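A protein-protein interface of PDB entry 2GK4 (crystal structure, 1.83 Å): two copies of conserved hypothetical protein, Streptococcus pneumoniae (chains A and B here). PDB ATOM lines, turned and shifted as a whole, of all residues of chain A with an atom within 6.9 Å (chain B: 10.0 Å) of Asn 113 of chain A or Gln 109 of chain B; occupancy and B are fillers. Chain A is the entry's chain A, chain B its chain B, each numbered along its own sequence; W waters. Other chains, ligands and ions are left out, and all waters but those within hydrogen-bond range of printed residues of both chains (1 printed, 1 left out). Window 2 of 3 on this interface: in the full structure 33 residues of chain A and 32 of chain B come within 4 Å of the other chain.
N of Leu 114 of chain A sits close to NE2 of Gln 109 of chain B, 3.0 Å away.
OD1 of Asn 113 of chain A sits close to N of Lys 115 of chain A (3.3 Å).
N of Leu 105 of chain B is in hydrogen-bond range of O of Val 133 of chain B (3.0 Å).
The backbone NH (N) of Asn 113 of chain A sits at hydrogen-bond distance from the side-chain hydroxyl (OG) of Ser 111 of chain A, 3.1 Å away.
Among the printed residues, merely in contact across the chains: Leu 114 of chain A with Leu 105 of chain B (3.5 Å), Leu 114 of chain A with Val 108 of chain B (3.6 Å), Val 108 of chain A with Leu 114 of chain B (3.7 Å), Asn 113 of chain A with Gln 109 of chain B (3.8 Å) and Lys 115 of chain A with Leu 105 of chain B (3.95 Å).
Gln 109 of chain B touches two residues of chain A.
No residue of chain B comes within 4 Å of Ser 111 of chain A.
No residue of chain B comes within 4 Å of Ser 112 of chain A.
Of chain B, only Leu 105, Val 108 and Gln 109 come within 4 Å of Leu 114 of chain A.
Of the printed residues of chain B, Val 108 of chain A touches Leu 114 (3.7 Å).
Of the printed residues of chain A, Leu 114 of chain B touches Val 108 (3.7 Å).
The nearest printed residue of chain A that does not touch Gln 109 of chain B is Lys 115 of chain A (4.5 Å).
Printed residues of chain A that touch a printed residue of chain B: Val 108, Asn 113, Leu 114 and Lys 115.
Along chain A the printed residues that touch a printed residue of chain B span positions 108 to 115.
Hydrophobic or aromatic side chains of chain B within 4 Å of the printed part of chain A: Leu 105, Val 108 and Leu 114.
Among the printed residues, no Asp or Glu carboxylate lies within 4 Å of a Lys or Arg side-chain nitrogen of the other chain.
Val 108 of chain A touches Leu 114 of chain B, and with the chains exchanged Leu 114 of chain A touches Val 108 of chain B.
Positions printed for both chains: 108, 110, 111, 112, 113, 114, 116 and 117.
Of the 6 pairs that touch across the chains among the printed residues, 2 have their exchanged pair printed and touching as well.
Water W1 bridges O of Ser 111 of chain A (2.5 Å) and OE1 of Gln 109 of chain B (3.2 Å).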
ATOM      1  N   VAL A 108     -23.264  18.487  31.496  1.00  0.00           N
ATOM      2  CA  VAL A 108     -23.759  18.340  30.117  1.00  0.00           C
ATOM      3  C   VAL A 108     -24.674  17.113  29.982  1.00  0.00           C
ATOM      4  O   VAL A 108     -25.741  17.177  29.373  1.00  0.00           O
ATOM      5  CB  VAL A 108     -22.612  18.266  29.088  1.00  0.00           C
ATOM      6  CG1 VAL A 108     -23.162  18.233  27.639  1.00  0.00           C
ATOM      7  CG2 VAL A 108     -21.673  19.498  29.258  1.00  0.00           C
ATOM      8  N   ALA A 110     -26.506  15.765  32.218  1.00  0.00           N
ATOM      9  CA  ALA A 110     -27.748  15.953  32.964  1.00  0.00           C
ATOM     10  C   ALA A 110     -28.706  16.917  32.266  1.00  0.00           C
ATOM     11  O   ALA A 110     -29.870  17.025  32.651  1.00  0.00           O
ATOM     12  CB  ALA A 110     -27.450  16.442  34.357  1.00  0.00           C
ATOM     13  N   SER A 111     -28.224  17.622  31.249  1.00  0.00           N
ATOM     14  CA  SER A 111     -29.034  18.640  30.580  1.00  0.00           C
ATOM     15  C   SER A 111     -30.069  18.007  29.645  1.00  0.00           C
ATOM     16  O   SER A 111     -29.807  16.986  29.002  1.00  0.00           O
ATOM     17  CB  SER A 111     -28.132  19.591  29.786  1.00  0.00           C
ATOM     18  OG  SER A 111     -28.882  20.425  28.918  1.00  0.00           O
ATOM     19  N   SER A 112     -31.234  18.631  29.563  1.00  0.00           N
ATOM     20  CA  SER A 112     -32.287  18.191  28.646  1.00  0.00           C
ATOM     21  C   SER A 112     -32.365  19.089  27.407  1.00  0.00           C
ATOM     22  O   SER A 112     -33.165  18.869  26.503  1.00  0.00           O
ATOM     23  CB  SER A 112     -33.639  18.150  29.376  1.00  0.00           C
ATOM     24  OG  SER A 112     -33.918  19.360  30.062  1.00  0.00           O
ATOM     25  N   ASN A 113     -31.523  20.117  27.363  1.00  0.00           N
ATOM     26  CA  ASN A 113     -31.451  20.965  26.193  1.00  0.00           C
ATOM     27  C   ASN A 113     -30.155  21.763  26.245  1.00  0.00           C
ATOM     28  O   ASN A 113     -30.015  22.699  27.029  1.00  0.00           O
ATOM     29  CB  ASN A 113     -32.660  21.905  26.090  1.00  0.00           C
ATOM     30  CG  ASN A 113     -32.711  22.653  24.761  1.00  0.00           C
ATOM     31  OD1 ASN A 113     -31.778  22.607  23.955  1.00  0.00           O
ATOM     32  ND2 ASN A 113     -33.822  23.329  24.516  1.00  0.00           N
ATOM     33  N   LEU A 114     -29.219  21.359  25.406  1.00  0.00           N
ATOM     34  CA  LEU A 114     -27.851  21.898  25.433  1.00  0.00           C
ATOM     35  C   LEU A 114     -27.764  23.381  25.067  1.00  0.00           C
ATOM     36  O   LEU A 114     -26.794  24.066  25.414  1.00  0.00           O
ATOM     37  CB  LEU A 114     -26.984  21.069  24.497  1.00  0.00           C
ATOM     38  CG  LEU A 114     -26.236  19.853  25.056  1.00  0.00           C
ATOM     39  CD1 LEU A 114     -26.871  19.159  26.217  1.00  0.00           C
ATOM     40  CD2 LEU A 114     -25.804  18.865  23.956  1.00  0.00           C
ATOM     41  N   LYS A 115     -28.778  23.881  24.363  1.00  0.00           N
ATOM     42  CA  LYS A 115     -28.818  25.308  24.040  1.00  0.00           C
ATOM     43  C   LYS A 115     -28.871  26.169  25.315  1.00  0.00           C
ATOM     44  O   LYS A 115     -28.474  27.346  25.284  1.00  0.00           O
ATOM     45  CB  LYS A 115     -29.974  25.612  23.072  1.00  0.00           C
ATOM     46  CG  LYS A 115     -29.793  24.882  21.741  1.00  0.00           C
ATOM     47  CD  LYS A 115     -30.733  25.338  20.597  1.00  0.00           C
ATOM     48  CE  LYS A 115     -30.452  24.482  19.347  1.00  0.00           C
ATOM     49  NZ  LYS A 115     -31.621  24.401  18.418  1.00  0.00           N
ATOM     50  N   GLU A 116     -29.310  25.578  26.437  1.00  0.00           N
ATOM     51  CA  GLU A 116     -29.342  26.288  27.733  1.00  0.00           C
ATOM     52  C   GLU A 116     -27.962  26.866  28.070  1.00  0.00           C
ATOM     53  O   GLU A 116     -27.867  27.922  28.677  1.00  0.00           O
ATOM     54  CB  GLU A 116     -29.822  25.401  28.895  1.00  0.00           C
ATOM     55  CG  GLU A 116     -28.765  24.410  29.464  1.00  0.00           C
ATOM     56  CD  GLU A 116     -29.250  23.581  30.689  1.00  0.00           C
ATOM     57  OE1 GLU A 116     -29.482  24.168  31.772  1.00  0.00           O
ATOM     58  OE2 GLU A 116     -29.353  22.336  30.584  1.00  0.00           O
ATOM     59  N   PHE A 117     -26.913  26.164  27.650  1.00  0.00           N
ATOM     60  CA  PHE A 117     -25.543  26.507  28.028  1.00  0.00           C
ATOM     61  C   PHE A 117     -25.038  27.776  27.354  1.00  0.00           C
ATOM     62  O   PHE A 117     -24.075  28.396  27.831  1.00  0.00           O
ATOM     63  CB  PHE A 117     -24.599  25.335  27.757  1.00  0.00           C
ATOM     64  CG  PHE A 117     -24.851  24.137  28.644  1.00  0.00           C
ATOM     65  CD1 PHE A 117     -25.198  22.917  28.096  1.00  0.00           C
ATOM     66  CD2 PHE A 117     -24.738  24.236  30.015  1.00  0.00           C
ATOM     67  CE1 PHE A 117     -25.440  21.807  28.909  1.00  0.00           C
ATOM     68  CE2 PHE A 117     -24.968  23.135  30.839  1.00  0.00           C
ATOM     69  CZ  PHE A 117     -25.324  21.919  30.283  1.00  0.00           C
ATOM     70  N   THR B 103     -16.970  19.276  17.608  1.00  0.00           N
ATOM     71  CA  THR B 103     -18.067  19.020  16.692  1.00  0.00           C
ATOM     72  C   THR B 103     -19.251  19.982  16.887  1.00  0.00           C
ATOM     73  O   THR B 103     -19.276  20.737  17.847  1.00  0.00           O
ATOM     74  CB  THR B 103     -18.507  17.542  16.780  1.00  0.00           C
ATOM     75  OG1 THR B 103     -19.336  17.226  15.655  1.00  0.00           O
ATOM     76  CG2 THR B 103     -19.232  17.249  18.122  1.00  0.00           C
ATOM     77  N   GLY B 104     -20.207  19.974  15.959  1.00  0.00           N
ATOM     78  CA  GLY B 104     -21.395  20.825  16.086  1.00  0.00           C
ATOM     79  C   GLY B 104     -22.307  20.366  17.221  1.00  0.00           C
ATOM     80  O   GLY B 104     -22.358  19.187  17.546  1.00  0.00           O
ATOM     81  N   LEU B 105     -23.008  21.317  17.833  1.00  0.00           N
ATOM     82  CA  LEU B 105     -23.941  21.049  18.926  1.00  0.00           C
ATOM     83  C   LEU B 105     -25.027  20.035  18.549  1.00  0.00           C
ATOM     84  O   LEU B 105     -25.423  19.222  19.373  1.00  0.00           O
ATOM     85  CB  LEU B 105     -24.614  22.347  19.357  1.00  0.00           C
ATOM     86  CG  LEU B 105     -25.583  22.337  20.546  1.00  0.00           C
ATOM     87  CD1 LEU B 105     -24.876  21.887  21.827  1.00  0.00           C
ATOM     88  CD2 LEU B 105     -26.159  23.728  20.708  1.00  0.00           C
ATOM     89  N   GLU B 106     -25.508  20.100  17.314  1.00  0.00           N
ATOM     90  CA  GLU B 106     -26.626  19.222  16.904  1.00  0.00           C
ATOM     91  C   GLU B 106     -26.242  17.748  16.955  1.00  0.00           C
ATOM     92  O   GLU B 106     -27.046  16.909  17.386  1.00  0.00           O
ATOM     93  CB  GLU B 106     -27.179  19.613  15.539  1.00  0.00           C
ATOM     94  CG  GLU B 106     -28.090  20.827  15.602  1.00  0.00           C
ATOM     95  CD  GLU B 106     -28.690  21.199  14.254  1.00  0.00           C
ATOM     96  OE1 GLU B 106     -28.391  22.310  13.763  1.00  0.00           O
ATOM     97  OE2 GLU B 106     -29.466  20.390  13.686  1.00  0.00           O
ATOM     98  N   GLU B 107     -25.004  17.437  16.568  1.00  0.00           N
ATOM     99  CA  GLU B 107     -24.504  16.073  16.681  1.00  0.00           C
ATOM    100  C   GLU B 107     -24.443  15.648  18.136  1.00  0.00           C
ATOM    101  O   GLU B 107     -24.763  14.516  18.472  1.00  0.00           O
ATOM    102  CB  GLU B 107     -23.130  15.914  16.026  1.00  0.00           C
ATOM    103  CG  GLU B 107     -22.475  14.562  16.352  1.00  0.00           C
ATOM    104  CD  GLU B 107     -21.366  14.145  15.392  1.00  0.00           C
ATOM    105  OE1 GLU B 107     -21.397  12.967  14.950  1.00  0.00           O
ATOM    106  OE2 GLU B 107     -20.470  14.969  15.086  1.00  0.00           O
ATOM    107  N   VAL B 108     -24.008  16.559  19.001  1.00  0.00           N
ATOM    108  CA  VAL B 108     -23.882  16.270  20.430  1.00  0.00           C
ATOM    109  C   VAL B 108     -25.270  16.080  21.033  1.00  0.00           C
ATOM    110  O   VAL B 108     -25.509  15.131  21.774  1.00  0.00           O
ATOM    111  CB  VAL B 108     -23.101  17.381  21.171  1.00  0.00           C
ATOM    112  CG1 VAL B 108     -23.007  17.077  22.667  1.00  0.00           C
ATOM    113  CG2 VAL B 108     -21.712  17.518  20.574  1.00  0.00           C
ATOM    114  N   GLN B 109     -26.183  16.978  20.687  1.00  0.00           N
ATOM    115  CA  GLN B 109     -27.539  16.907  21.179  1.00  0.00           C
ATOM    116  C   GLN B 109     -28.147  15.554  20.810  1.00  0.00           C
ATOM    117  O   GLN B 109     -28.809  14.925  21.645  1.00  0.00           O
ATOM    118  CB  GLN B 109     -28.369  18.045  20.584  1.00  0.00           C
ATOM    119  CG  GLN B 109     -29.799  18.139  21.128  1.00  0.00           C
ATOM    120  CD  GLN B 109     -29.850  18.381  22.626  1.00  0.00           C
ATOM    121  OE1 GLN B 109     -30.151  17.472  23.394  1.00  0.00           O
ATOM    122  NE2 GLN B 109     -29.575  19.603  23.044  1.00  0.00           N
ATOM    123  N   ALA B 110     -27.888  15.114  19.577  1.00  0.00           N
ATOM    124  CA  ALA B 110     -28.498  13.893  19.034  1.00  0.00           C
ATOM    125  C   ALA B 110     -28.019  12.609  19.708  1.00  0.00           C
ATOM    126  O   ALA B 110     -28.725  11.590  19.702  1.00  0.00           O
ATOM    127  CB  ALA B 110     -28.279  13.819  17.531  1.00  0.00           C
ATOM    128  N   SER B 111     -26.822  12.662  20.283  1.00  0.00           N
ATOM    129  CA  SER B 111     -26.186  11.502  20.890  1.00  0.00           C
ATOM    130  C   SER B 111     -26.956  10.953  22.081  1.00  0.00           C
ATOM    131  O   SER B 111     -27.391  11.703  22.962  1.00  0.00           O
ATOM    132  CB  SER B 111     -24.764  11.847  21.327  1.00  0.00           C
ATOM    133  OG  SER B 111     -24.100  10.707  21.832  1.00  0.00           O
ATOM    134  N   SER B 112     -27.106   9.633  22.099  1.00  0.00           N
ATOM    135  CA  SER B 112     -27.678   8.935  23.242  1.00  0.00           C
ATOM    136  C   SER B 112     -26.591   8.598  24.268  1.00  0.00           C
ATOM    137  O   SER B 112     -26.889   8.067  25.345  1.00  0.00           O
ATOM    138  CB  SER B 112     -28.380   7.655  22.780  1.00  0.00           C
ATOM    139  OG  SER B 112     -27.432   6.635  22.505  1.00  0.00           O
ATOM    140  N   ASN B 113     -25.333   8.892  23.930  1.00  0.00           N
ATOM    141  CA  ASN B 113     -24.197   8.565  24.795  1.00  0.00           C
ATOM    142  C   ASN B 113     -22.941   9.399  24.501  1.00  0.00           C
ATOM    143  O   ASN B 113     -22.238   9.147  23.522  1.00  0.00           O
ATOM    144  CB  ASN B 113     -23.869   7.070  24.696  1.00  0.00           C
ATOM    145  CG  ASN B 113     -22.718   6.666  25.599  1.00  0.00           C
ATOM    146  OD1 ASN B 113     -22.408   7.348  26.580  1.00  0.00           O
ATOM    147  ND2 ASN B 113     -22.070   5.555  25.266  1.00  0.00           N
ATOM    148  N   LEU B 114     -22.665  10.369  25.374  1.00  0.00           N
ATOM    149  CA  LEU B 114     -21.591  11.358  25.172  1.00  0.00           C
ATOM    150  C   LEU B 114     -20.178  10.792  25.252  1.00  0.00           C
ATOM    151  O   LEU B 114     -19.240  11.343  24.663  1.00  0.00           O
ATOM    152  CB  LEU B 114     -21.753  12.521  26.157  1.00  0.00           C
ATOM    153  CG  LEU B 114     -22.538  13.728  25.641  1.00  0.00           C
ATOM    154  CD1 LEU B 114     -23.675  13.323  24.748  1.00  0.00           C
ATOM    155  CD2 LEU B 114     -23.022  14.603  26.785  1.00  0.00           C
ATOM    156  N   GLU B 116     -19.077   8.545  23.690  1.00  0.00           N
ATOM    157  CA  GLU B 116     -18.685   8.197  22.321  1.00  0.00           C
ATOM    158  C   GLU B 116     -17.672   9.170  21.716  1.00  0.00           C
ATOM    159  O   GLU B 116     -16.756   8.752  21.007  1.00  0.00           O
ATOM    160  CB  GLU B 116     -19.904   8.049  21.391  1.00  0.00           C
ATOM    161  CG  GLU B 116     -20.644   9.357  21.037  1.00  0.00           C
ATOM    162  CD  GLU B 116     -21.351   9.311  19.684  1.00  0.00           C
ATOM    163  OE1 GLU B 116     -20.679   9.006  18.672  1.00  0.00           O
ATOM    164  OE2 GLU B 116     -22.574   9.600  19.623  1.00  0.00           O
ATOM    165  N   PHE B 117     -17.830  10.462  22.010  1.00  0.00           N
ATOM    166  CA  PHE B 117     -17.007  11.510  21.392  1.00  0.00           C
ATOM    167  C   PHE B 117     -15.568  11.498  21.893  1.00  0.00           C
ATOM    168  O   PHE B 117     -14.740  12.278  21.422  1.00  0.00           O
ATOM    169  CB  PHE B 117     -17.628  12.896  21.621  1.00  0.00           C
ATOM    170  CG  PHE B 117     -19.003  13.040  21.045  1.00  0.00           C
ATOM    171  CD1 PHE B 117     -20.115  13.070  21.872  1.00  0.00           C
ATOM    172  CD2 PHE B 117     -19.190  13.121  19.673  1.00  0.00           C
ATOM    173  CE1 PHE B 117     -21.386  13.196  21.339  1.00  0.00           C
ATOM    174  CE2 PHE B 117     -20.473  13.243  19.132  1.00  0.00           C
ATOM    175  CZ  PHE B 117     -21.563  13.280  19.963  1.00  0.00           C
ATOM    176  N   VAL B 133     -23.129  26.574  16.740  1.00  0.00           N
ATOM    177  CA  VAL B 133     -22.426  26.301  17.995  1.00  0.00           C
ATOM    178  C   VAL B 133     -21.522  25.102  17.808  1.00  0.00           C
ATOM    179  O   VAL B 133     -21.931  24.097  17.203  1.00  0.00           O
ATOM    180  CB  VAL B 133     -23.428  26.036  19.153  1.00  0.00           C
ATOM    181  CG1 VAL B 133     -22.701  25.591  20.445  1.00  0.00           C
ATOM    182  CG2 VAL B 133     -24.290  27.261  19.387  1.00  0.00           C
ATOM    183  N   GLN B 134     -20.306  25.215  18.339  1.00  0.00           N
ATOM    184  CA  GLN B 134     -19.375  24.098  18.404  1.00  0.00           C
ATOM    185  C   GLN B 134     -19.179  23.655  19.842  1.00  0.00           C
ATOM    186  O   GLN B 134     -19.395  24.434  20.780  1.00  0.00           O
ATOM    187  CB  GLN B 134     -18.028  24.471  17.792  1.00  0.00           C
ATOM    188  CG  GLN B 134     -18.067  24.713  16.306  1.00  0.00           C
ATOM    189  CD  GLN B 134     -18.254  23.458  15.475  1.00  0.00           C
ATOM    190  OE1 GLN B 134     -19.167  23.379  14.643  1.00  0.00           O
ATOM    191  NE2 GLN B 134     -17.377  22.496  15.659  1.00  0.00           N
ATOM    192  N   VAL B 135     -18.805  22.390  20.001  1.00  0.00           N
ATOM    193  CA  VAL B 135     -18.584  21.786  21.309  1.00  0.00           C
ATOM    194  C   VAL B 135     -17.221  21.101  21.279  1.00  0.00           C
ATOM    195  O   VAL B 135     -16.957  20.296  20.398  1.00  0.00           O
ATOM    196  CB  VAL B 135     -19.688  20.733  21.643  1.00  0.00           C
ATOM    197  CG1 VAL B 135     -19.500  20.172  23.033  1.00  0.00           C
ATOM    198  CG2 VAL B 135     -21.086  21.334  21.472  1.00  0.00           C
ATOM    199  N   PHE B 137     -14.603  18.702  23.316  1.00  0.00           N
ATOM    200  CA  PHE B 137     -14.388  17.775  24.434  1.00  0.00           C
ATOM    201  C   PHE B 137     -12.903  17.679  24.752  1.00  0.00           C
ATOM    202  O   PHE B 137     -12.087  17.446  23.858  1.00  0.00           O
ATOM    203  CB  PHE B 137     -14.928  16.380  24.090  1.00  0.00           C
ATOM    204  CG  PHE B 137     -16.418  16.331  23.915  1.00  0.00           C
ATOM    205  CD1 PHE B 137     -16.999  16.654  22.698  1.00  0.00           C
ATOM    206  CD2 PHE B 137     -17.250  15.936  24.975  1.00  0.00           C
ATOM    207  CE1 PHE B 137     -18.407  16.623  22.542  1.00  0.00           C
ATOM    208  CE2 PHE B 137     -18.652  15.889  24.817  1.00  0.00           C
ATOM    209  CZ  PHE B 137     -19.221  16.224  23.600  1.00  0.00           C
HETATM  210  O   HOH W   1     -29.785  16.900  26.540  1.00  0.00           O
